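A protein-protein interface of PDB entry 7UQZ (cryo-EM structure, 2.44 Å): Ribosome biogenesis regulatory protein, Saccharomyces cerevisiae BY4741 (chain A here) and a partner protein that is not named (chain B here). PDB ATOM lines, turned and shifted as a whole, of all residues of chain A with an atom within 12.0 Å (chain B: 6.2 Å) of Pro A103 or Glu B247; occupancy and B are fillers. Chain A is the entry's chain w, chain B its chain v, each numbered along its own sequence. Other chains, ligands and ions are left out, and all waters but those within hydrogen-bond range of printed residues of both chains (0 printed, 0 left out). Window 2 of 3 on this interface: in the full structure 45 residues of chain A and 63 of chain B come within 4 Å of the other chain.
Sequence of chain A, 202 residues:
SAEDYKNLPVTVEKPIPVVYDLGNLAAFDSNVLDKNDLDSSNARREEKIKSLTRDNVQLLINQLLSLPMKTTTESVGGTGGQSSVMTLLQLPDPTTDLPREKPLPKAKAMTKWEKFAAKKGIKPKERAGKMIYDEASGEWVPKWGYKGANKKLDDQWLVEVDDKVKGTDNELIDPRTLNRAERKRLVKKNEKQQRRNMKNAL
The guanidinium group (NH1) of Arg A100 is in hydrogen-bond range of the backbone carbonyl oxygen (O) of Lys B22, at 2.9 Å.
OE2 of Glu B25 lies within salt-bridge range of NH2 of Arg A100 (3.6 Å).
The side-chain carboxylate (OE1) of Glu B25 lies within salt-bridge range of the side-chain amino group (NZ) of Lys A102 (3.7 Å).
O of Glu A101 is in hydrogen-bond range of N of Gly B107 (2.8 Å).
The backbone carbonyl oxygen (O) of Ala B248 lies close to the backbone NH (N) of Arg A100, 3.3 Å away.
The side-chain carboxylate (OE2) of Glu A101 lies close to the side-chain carboxylate (OE1) of Glu B25.
The backbone NH (N) of Lys B22 is in hydrogen-bond range of the side-chain carboxylate (OE2) of Glu B25, 3.3 Å away.
A ring nitrogen (ND1) of His B249 sits at hydrogen-bond distance from the backbone carbonyl oxygen (O) of Val B245 (2.8 Å).
The guanidinium group (NE) of Arg A100 lies within hydrogen-bond range of the backbone carbonyl oxygen (O) of Lys A102 (2.9 Å).
The guanidinium group (NH2) of Arg A100 is in hydrogen-bond range of the backbone carbonyl oxygen (O) of Pro A103 (3.0 Å).
Among the printed residues, merely in contact across the chains: Arg A100 with Phe B106 (3.1 Å), Asp A97 with His B249 (3.2 Å), Pro A103 with Phe B106 (3.4 Å), Pro A103 with Ala B21 (3.5 Å), Lys A102 with Phe B106 (3.6 Å), Glu A101 with Phe B106 (3.6 Å), Pro A99 with Ala B248 (3.7 Å), Pro A103 with Glu B247 (3.7 Å), Lys A102 with Ala B21 (3.7 Å) and Pro A103 with Gly B107 (3.9 Å).
Printed residues of chain A within 4 Å of Ala B21: Lys A102 and Pro A103.
Phe B106 touches four residues of chain A.
Gly B107 touches just these residues of chain A: Glu A101 (2.8 Å) and Pro A103 (3.9 Å).
No residue of chain A comes within 4 Å of Asp B243.
No residue of chain A comes within 4 Å of Val B245.
No residue of chain A comes within 4 Å of Thr B246.
Of the printed residues of chain A, Lys B22 touches Arg A100 (2.9 Å).
Printed residues of chain A within 4 Å of His B249: Asp A97 (3.2 Å).
Of the printed residues of chain A, Glu B25 touches Arg A100, Glu A101 and Lys A102.
Ala A107 touches none of the printed residues of chain B.
Leu A98 touches none of the printed residues of chain B.
The nearest residue of chain A that does not touch Glu B247 is Leu A104 (5.4 Å).
The nearest printed residue of chain B that does not touch Glu A101 is Ala B248 (6.5 Å).
Of the 14 printed residues of chain B, 8 touch a printed residue of chain A.
Hydrophobic or aromatic side chains of chain B that line the printed part of chain A: Ala B21, Phe B106, Ala B248 and His B249.
Along chain A the printed residues that touch a printed residue of chain B span positions 97 to 103.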
ATOM      1  N   ASP A  97      -1.002  29.619  -9.793  1.00  0.00           N
ATOM      2  CA  ASP A  97      -1.209  28.266 -10.286  1.00  0.00           C
ATOM      3  C   ASP A  97       0.094  27.482 -10.193  1.00  0.00           C
ATOM      4  O   ASP A  97       1.141  27.950 -10.650  1.00  0.00           O
ATOM      5  CB  ASP A  97      -1.723  28.284 -11.727  1.00  0.00           C
ATOM      6  CG  ASP A  97      -0.890  29.168 -12.633  1.00  0.00           C
ATOM      7  OD1 ASP A  97      -0.307  30.153 -12.131  1.00  0.00           O
ATOM      8  OD2 ASP A  97      -0.817  28.879 -13.845  1.00  0.00           O
ATOM      9  N   LEU A  98       0.022  26.297  -9.598  1.00  0.00           N
ATOM     10  CA  LEU A  98       1.174  25.434  -9.404  1.00  0.00           C
ATOM     11  C   LEU A  98       0.879  24.053  -9.965  1.00  0.00           C
ATOM     12  O   LEU A  98      -0.271  23.602  -9.940  1.00  0.00           O
ATOM     13  CB  LEU A  98       1.532  25.318  -7.915  1.00  0.00           C
ATOM     14  CG  LEU A  98       1.804  26.626  -7.170  1.00  0.00           C
ATOM     15  CD1 LEU A  98       2.063  26.363  -5.695  1.00  0.00           C
ATOM     16  CD2 LEU A  98       2.969  27.373  -7.802  1.00  0.00           C
ATOM     17  N   PRO A  99       1.891  23.366 -10.489  1.00  0.00           N
ATOM     18  CA  PRO A  99       1.665  22.019 -11.022  1.00  0.00           C
ATOM     19  C   PRO A  99       1.340  21.018  -9.926  1.00  0.00           C
ATOM     20  O   PRO A  99       1.858  21.086  -8.809  1.00  0.00           O
ATOM     21  CB  PRO A  99       2.995  21.682 -11.707  1.00  0.00           C
ATOM     22  CG  PRO A  99       3.998  22.541 -11.023  1.00  0.00           C
ATOM     23  CD  PRO A  99       3.279  23.814 -10.695  1.00  0.00           C
ATOM     24  N   ARG A 100       0.470  20.072 -10.266  1.00  0.00           N
ATOM     25  CA  ARG A 100       0.139  18.999  -9.345  1.00  0.00           C
ATOM     26  C   ARG A 100       1.286  17.997  -9.261  1.00  0.00           C
ATOM     27  O   ARG A 100       2.119  17.884 -10.163  1.00  0.00           O
ATOM     28  CB  ARG A 100      -1.138  18.286  -9.783  1.00  0.00           C
ATOM     29  CG  ARG A 100      -2.311  19.206 -10.073  1.00  0.00           C
ATOM     30  CD  ARG A 100      -3.591  18.638  -9.491  1.00  0.00           C
ATOM     31  NE  ARG A 100      -3.698  17.200  -9.705  1.00  0.00           N
ATOM     32  CZ  ARG A 100      -4.563  16.414  -9.080  1.00  0.00           C
ATOM     33  NH1 ARG A 100      -5.418  16.896  -8.193  1.00  0.00           N
ATOM     34  NH2 ARG A 100      -4.568  15.113  -9.347  1.00  0.00           N
ATOM     35  N   GLU A 101       1.328  17.267  -8.148  1.00  0.00           N
ATOM     36  CA  GLU A 101       2.286  16.180  -8.009  1.00  0.00           C
ATOM     37  C   GLU A 101       1.862  14.927  -8.765  1.00  0.00           C
ATOM     38  O   GLU A 101       2.719  14.102  -9.096  1.00  0.00           O
ATOM     39  CB  GLU A 101       2.496  15.851  -6.531  1.00  0.00           C
ATOM     40  CG  GLU A 101       1.217  15.758  -5.724  1.00  0.00           C
ATOM     41  CD  GLU A 101       1.476  15.791  -4.233  1.00  0.00           C
ATOM     42  OE1 GLU A 101       2.660  15.760  -3.839  1.00  0.00           O
ATOM     43  OE2 GLU A 101       0.500  15.854  -3.457  1.00  0.00           O
ATOM     44  N   LYS A 102       0.572  14.769  -9.038  1.00  0.00           N
ATOM     45  CA  LYS A 102       0.042  13.627  -9.766  1.00  0.00           C
ATOM     46  C   LYS A 102      -1.089  14.094 -10.669  1.00  0.00           C
ATOM     47  O   LYS A 102      -1.767  15.080 -10.356  1.00  0.00           O
ATOM     48  CB  LYS A 102      -0.464  12.534  -8.811  1.00  0.00           C
ATOM     49  CG  LYS A 102       0.642  11.697  -8.186  1.00  0.00           C
ATOM     50  CD  LYS A 102       0.080  10.617  -7.282  1.00  0.00           C
ATOM     51  CE  LYS A 102      -0.408  11.192  -5.962  1.00  0.00           C
ATOM     52  NZ  LYS A 102       0.717  11.539  -5.049  1.00  0.00           N
ATOM     53  N   PRO A 103      -1.314  13.416 -11.793  1.00  0.00           N
ATOM     54  CA  PRO A 103      -2.412  13.804 -12.685  1.00  0.00           C
ATOM     55  C   PRO A 103      -3.769  13.516 -12.060  1.00  0.00           C
ATOM     56  O   PRO A 103      -3.901  12.778 -11.083  1.00  0.00           O
ATOM     57  CB  PRO A 103      -2.178  12.948 -13.935  1.00  0.00           C
ATOM     58  CG  PRO A 103      -1.368  11.794 -13.454  1.00  0.00           C
ATOM     59  CD  PRO A 103      -0.488  12.343 -12.375  1.00  0.00           C
ATOM     60  N   LEU A 104      -4.791  14.139 -12.644  1.00  0.00           N
ATOM     61  CA  LEU A 104      -6.155  13.931 -12.182  1.00  0.00           C
ATOM     62  C   LEU A 104      -6.579  12.484 -12.422  1.00  0.00           C
ATOM     63  O   LEU A 104      -6.169  11.872 -13.414  1.00  0.00           O
ATOM     64  CB  LEU A 104      -7.117  14.876 -12.898  1.00  0.00           C
ATOM     65  CG  LEU A 104      -7.077  16.357 -12.525  1.00  0.00           C
ATOM     66  CD1 LEU A 104      -7.994  17.146 -13.439  1.00  0.00           C
ATOM     67  CD2 LEU A 104      -7.476  16.555 -11.075  1.00  0.00           C
ATOM     68  N   PRO A 105      -7.385  11.908 -11.531  1.00  0.00           N
ATOM     69  CA  PRO A 105      -7.832  10.524 -11.726  1.00  0.00           C
ATOM     70  C   PRO A 105      -8.779  10.415 -12.913  1.00  0.00           C
ATOM     71  O   PRO A 105      -9.784  11.123 -12.991  1.00  0.00           O
ATOM     72  CB  PRO A 105      -8.542  10.188 -10.408  1.00  0.00           C
ATOM     73  CG  PRO A 105      -8.060  11.218  -9.431  1.00  0.00           C
ATOM     74  CD  PRO A 105      -7.819  12.451 -10.234  1.00  0.00           C
ATOM     75  N   LYS A 106      -8.445   9.522 -13.840  1.00  0.00           N
ATOM     76  CA  LYS A 106      -9.298   9.283 -14.993  1.00  0.00           C
ATOM     77  C   LYS A 106     -10.547   8.509 -14.587  1.00  0.00           C
ATOM     78  O   LYS A 106     -10.539   7.726 -13.632  1.00  0.00           O
ATOM     79  CB  LYS A 106      -8.535   8.516 -16.072  1.00  0.00           C
ATOM     80  CG  LYS A 106      -7.344   9.266 -16.648  1.00  0.00           C
ATOM     81  CD  LYS A 106      -6.596   8.414 -17.658  1.00  0.00           C
ATOM     82  CE  LYS A 106      -7.497   7.999 -18.810  1.00  0.00           C
ATOM     83  NZ  LYS A 106      -7.987   9.166 -19.595  1.00  0.00           N
ATOM     84  N   ALA A 107     -11.632   8.740 -15.322  1.00  0.00           N
ATOM     85  CA  ALA A 107     -12.874   8.022 -15.071  1.00  0.00           C
ATOM     86  C   ALA A 107     -12.750   6.578 -15.540  1.00  0.00           C
ATOM     87  O   ALA A 107     -12.260   6.312 -16.642  1.00  0.00           O
ATOM     88  CB  ALA A 107     -14.039   8.712 -15.776  1.00  0.00           C
ATOM     89  N   ALA B  21      -3.535   9.011  -6.525  1.00  0.00           N
ATOM     90  CA  ALA B  21      -3.943  10.361  -6.885  1.00  0.00           C
ATOM     91  C   ALA B  21      -5.317  10.693  -6.307  1.00  0.00           C
ATOM     92  O   ALA B  21      -6.123   9.812  -5.993  1.00  0.00           O
ATOM     93  CB  ALA B  21      -3.962  10.527  -8.403  1.00  0.00           C
ATOM     94  N   LYS B  22      -5.582  11.992  -6.177  1.00  0.00           N
ATOM     95  CA  LYS B  22      -6.832  12.461  -5.593  1.00  0.00           C
ATOM     96  C   LYS B  22      -7.134  13.862  -6.106  1.00  0.00           C
ATOM     97  O   LYS B  22      -6.269  14.540  -6.664  1.00  0.00           O
ATOM     98  CB  LYS B  22      -6.772  12.442  -4.064  1.00  0.00           C
ATOM     99  CG  LYS B  22      -5.460  12.937  -3.485  1.00  0.00           C
ATOM    100  CD  LYS B  22      -5.324  12.526  -2.028  1.00  0.00           C
ATOM    101  CE  LYS B  22      -5.443  11.016  -1.875  1.00  0.00           C
ATOM    102  NZ  LYS B  22      -5.332  10.582  -0.457  1.00  0.00           N
ATOM    103  N   GLU B  25      -4.962  17.179  -3.559  1.00  0.00           N
ATOM    104  CA  GLU B  25      -3.701  16.520  -3.269  1.00  0.00           C
ATOM    105  C   GLU B  25      -3.220  16.863  -1.863  1.00  0.00           C
ATOM    106  O   GLU B  25      -3.632  17.855  -1.254  1.00  0.00           O
ATOM    107  CB  GLU B  25      -2.638  16.910  -4.297  1.00  0.00           C
ATOM    108  CG  GLU B  25      -2.770  16.195  -5.634  1.00  0.00           C
ATOM    109  CD  GLU B  25      -2.433  14.716  -5.547  1.00  0.00           C
ATOM    110  OE1 GLU B  25      -1.709  14.318  -4.610  1.00  0.00           O
ATOM    111  OE2 GLU B  25      -2.893  13.947  -6.417  1.00  0.00           O
ATOM    112  N   PHE B 106       6.180  15.432 -11.661  1.00  0.00           N
ATOM    113  CA  PHE B 106       4.746  15.296 -11.881  1.00  0.00           C
ATOM    114  C   PHE B 106       4.458  13.870 -12.321  1.00  0.00           C
ATOM    115  O   PHE B 106       4.915  13.444 -13.387  1.00  0.00           O
ATOM    116  CB  PHE B 106       4.256  16.295 -12.932  1.00  0.00           C
ATOM    117  CG  PHE B 106       2.907  15.963 -13.509  1.00  0.00           C
ATOM    118  CD1 PHE B 106       1.751  16.181 -12.779  1.00  0.00           C
ATOM    119  CD2 PHE B 106       2.794  15.449 -14.791  1.00  0.00           C
ATOM    120  CE1 PHE B 106       0.509  15.883 -13.309  1.00  0.00           C
ATOM    121  CE2 PHE B 106       1.556  15.147 -15.328  1.00  0.00           C
ATOM    122  CZ  PHE B 106       0.413  15.366 -14.585  1.00  0.00           C
ATOM    123  N   GLY B 107       3.697  13.143 -11.509  1.00  0.00           N
ATOM    124  CA  GLY B 107       3.337  11.773 -11.841  1.00  0.00           C
ATOM    125  C   GLY B 107       4.512  10.822 -11.900  1.00  0.00           C
ATOM    126  O   GLY B 107       4.577   9.978 -12.802  1.00  0.00           O
ATOM    127  N   PRO B 242       5.068  21.581 -23.044  1.00  0.00           N
ATOM    128  CA  PRO B 242       3.781  22.296 -22.940  1.00  0.00           C
ATOM    129  C   PRO B 242       2.596  21.406 -22.603  1.00  0.00           C
ATOM    130  O   PRO B 242       1.722  21.810 -21.821  1.00  0.00           O
ATOM    131  CB  PRO B 242       3.631  22.933 -24.328  1.00  0.00           C
ATOM    132  CG  PRO B 242       5.024  23.059 -24.839  1.00  0.00           C
ATOM    133  CD  PRO B 242       5.754  21.861 -24.317  1.00  0.00           C
ATOM    134  N   ASP B 243       2.539  20.198 -23.168  1.00  0.00           N
ATOM    135  CA  ASP B 243       1.433  19.300 -22.854  1.00  0.00           C
ATOM    136  C   ASP B 243       1.500  18.841 -21.404  1.00  0.00           C
ATOM    137  O   ASP B 243       0.464  18.680 -20.749  1.00  0.00           O
ATOM    138  CB  ASP B 243       1.429  18.106 -23.810  1.00  0.00           C
ATOM    139  CG  ASP B 243       2.581  17.156 -23.567  1.00  0.00           C
ATOM    140  OD1 ASP B 243       3.697  17.637 -23.275  1.00  0.00           O
ATOM    141  OD2 ASP B 243       2.368  15.930 -23.658  1.00  0.00           O
ATOM    142  N   MET B 244       2.713  18.650 -20.879  1.00  0.00           N
ATOM    143  CA  MET B 244       2.868  18.323 -19.466  1.00  0.00           C
ATOM    144  C   MET B 244       2.441  19.489 -18.586  1.00  0.00           C
ATOM    145  O   MET B 244       1.848  19.283 -17.521  1.00  0.00           O
ATOM    146  CB  MET B 244       4.314  17.924 -19.178  1.00  0.00           C
ATOM    147  CG  MET B 244       4.491  17.083 -17.927  1.00  0.00           C
ATOM    148  SD  MET B 244       6.213  16.636 -17.634  1.00  0.00           S
ATOM    149  CE  MET B 244       6.017  15.278 -16.486  1.00  0.00           C
ATOM    150  N   VAL B 245       2.725  20.720 -19.021  1.00  0.00           N
ATOM    151  CA  VAL B 245       2.281  21.902 -18.282  1.00  0.00           C
ATOM    152  C   VAL B 245       0.759  21.950 -18.225  1.00  0.00           C
ATOM    153  O   VAL B 245       0.165  22.199 -17.169  1.00  0.00           O
ATOM    154  CB  VAL B 245       2.861  23.180 -18.916  1.00  0.00           C
ATOM    155  CG1 VAL B 245       2.230  24.419 -18.301  1.00  0.00           C
ATOM    156  CG2 VAL B 245       4.363  23.221 -18.743  1.00  0.00           C
ATOM    157  N   THR B 246       0.106  21.701 -19.364  1.00  0.00           N
ATOM    158  CA  THR B 246      -1.355  21.699 -19.394  1.00  0.00           C
ATOM    159  C   THR B 246      -1.929  20.588 -18.517  1.00  0.00           C
ATOM    160  O   THR B 246      -2.888  20.812 -17.767  1.00  0.00           O
ATOM    161  CB  THR B 246      -1.860  21.554 -20.829  1.00  0.00           C
ATOM    162  OG1 THR B 246      -1.348  20.344 -21.399  1.00  0.00           O
ATOM    163  CG2 THR B 246      -1.420  22.740 -21.673  1.00  0.00           C
ATOM    164  N   GLU B 247      -1.343  19.390 -18.591  1.00  0.00           N
ATOM    165  CA  GLU B 247      -1.833  18.266 -17.797  1.00  0.00           C
ATOM    166  C   GLU B 247      -1.652  18.517 -16.305  1.00  0.00           C
ATOM    167  O   GLU B 247      -2.493  18.108 -15.496  1.00  0.00           O
ATOM    168  CB  GLU B 247      -1.120  16.979 -18.215  1.00  0.00           C
ATOM    169  CG  GLU B 247      -1.672  15.724 -17.557  1.00  0.00           C
ATOM    170  CD  GLU B 247      -0.863  14.484 -17.882  1.00  0.00           C
ATOM    171  OE1 GLU B 247       0.196  14.614 -18.533  1.00  0.00           O
ATOM    172  OE2 GLU B 247      -1.285  13.377 -17.486  1.00  0.00           O
ATOM    173  N   ALA B 248      -0.561  19.181 -15.922  1.00  0.00           N
ATOM    174  CA  ALA B 248      -0.341  19.501 -14.518  1.00  0.00           C
ATOM    175  C   ALA B 248      -1.220  20.652 -14.042  1.00  0.00           C
ATOM    176  O   ALA B 248      -1.538  20.727 -12.851  1.00  0.00           O
ATOM    177  CB  ALA B 248       1.131  19.833 -14.280  1.00  0.00           C
ATOM    178  N   HIS B 249      -1.609  21.558 -14.936  1.00  0.00           N
ATOM    179  CA  HIS B 249      -2.443  22.691 -14.560  1.00  0.00           C
ATOM    180  C   HIS B 249      -3.928  22.447 -14.798  1.00  0.00           C
ATOM    181  O   HIS B 249      -4.729  23.369 -14.618  1.00  0.00           O
ATOM    182  CB  HIS B 249      -1.987  23.948 -15.301  1.00  0.00           C
ATOM    183  CG  HIS B 249      -0.706  24.520 -14.779  1.00  0.00           C
ATOM    184  ND1 HIS B 249       0.505  23.877 -14.911  1.00  0.00           N
ATOM    185  CD2 HIS B 249      -0.450  25.672 -14.114  1.00  0.00           C
ATOM    186  CE1 HIS B 249       1.454  24.610 -14.355  1.00  0.00           C
ATOM    187  NE2 HIS B 249       0.900  25.704 -13.865  1.00  0.00           N
ATOM    188  N   LYS B 250      -4.311  21.241 -15.214  1.00  0.00           N
ATOM    189  CA  LYS B 250      -5.729  20.912 -15.304  1.00  0.00           C
ATOM    190  C   LYS B 250      -6.380  20.931 -13.924  1.00  0.00           C
ATOM    191  O   LYS B 250      -5.767  20.574 -12.915  1.00  0.00           O
ATOM    192  CB  LYS B 250      -5.924  19.539 -15.952  1.00  0.00           C
ATOM    193  CG  LYS B 250      -5.862  19.556 -17.470  1.00  0.00           C
ATOM    194  CD  LYS B 250      -6.180  18.190 -18.054  1.00  0.00           C
ATOM    195  CE  LYS B 250      -6.207  18.233 -19.574  1.00  0.00           C
ATOM    196  NZ  LYS B 250      -4.885  18.608 -20.147  1.00  0.00           N
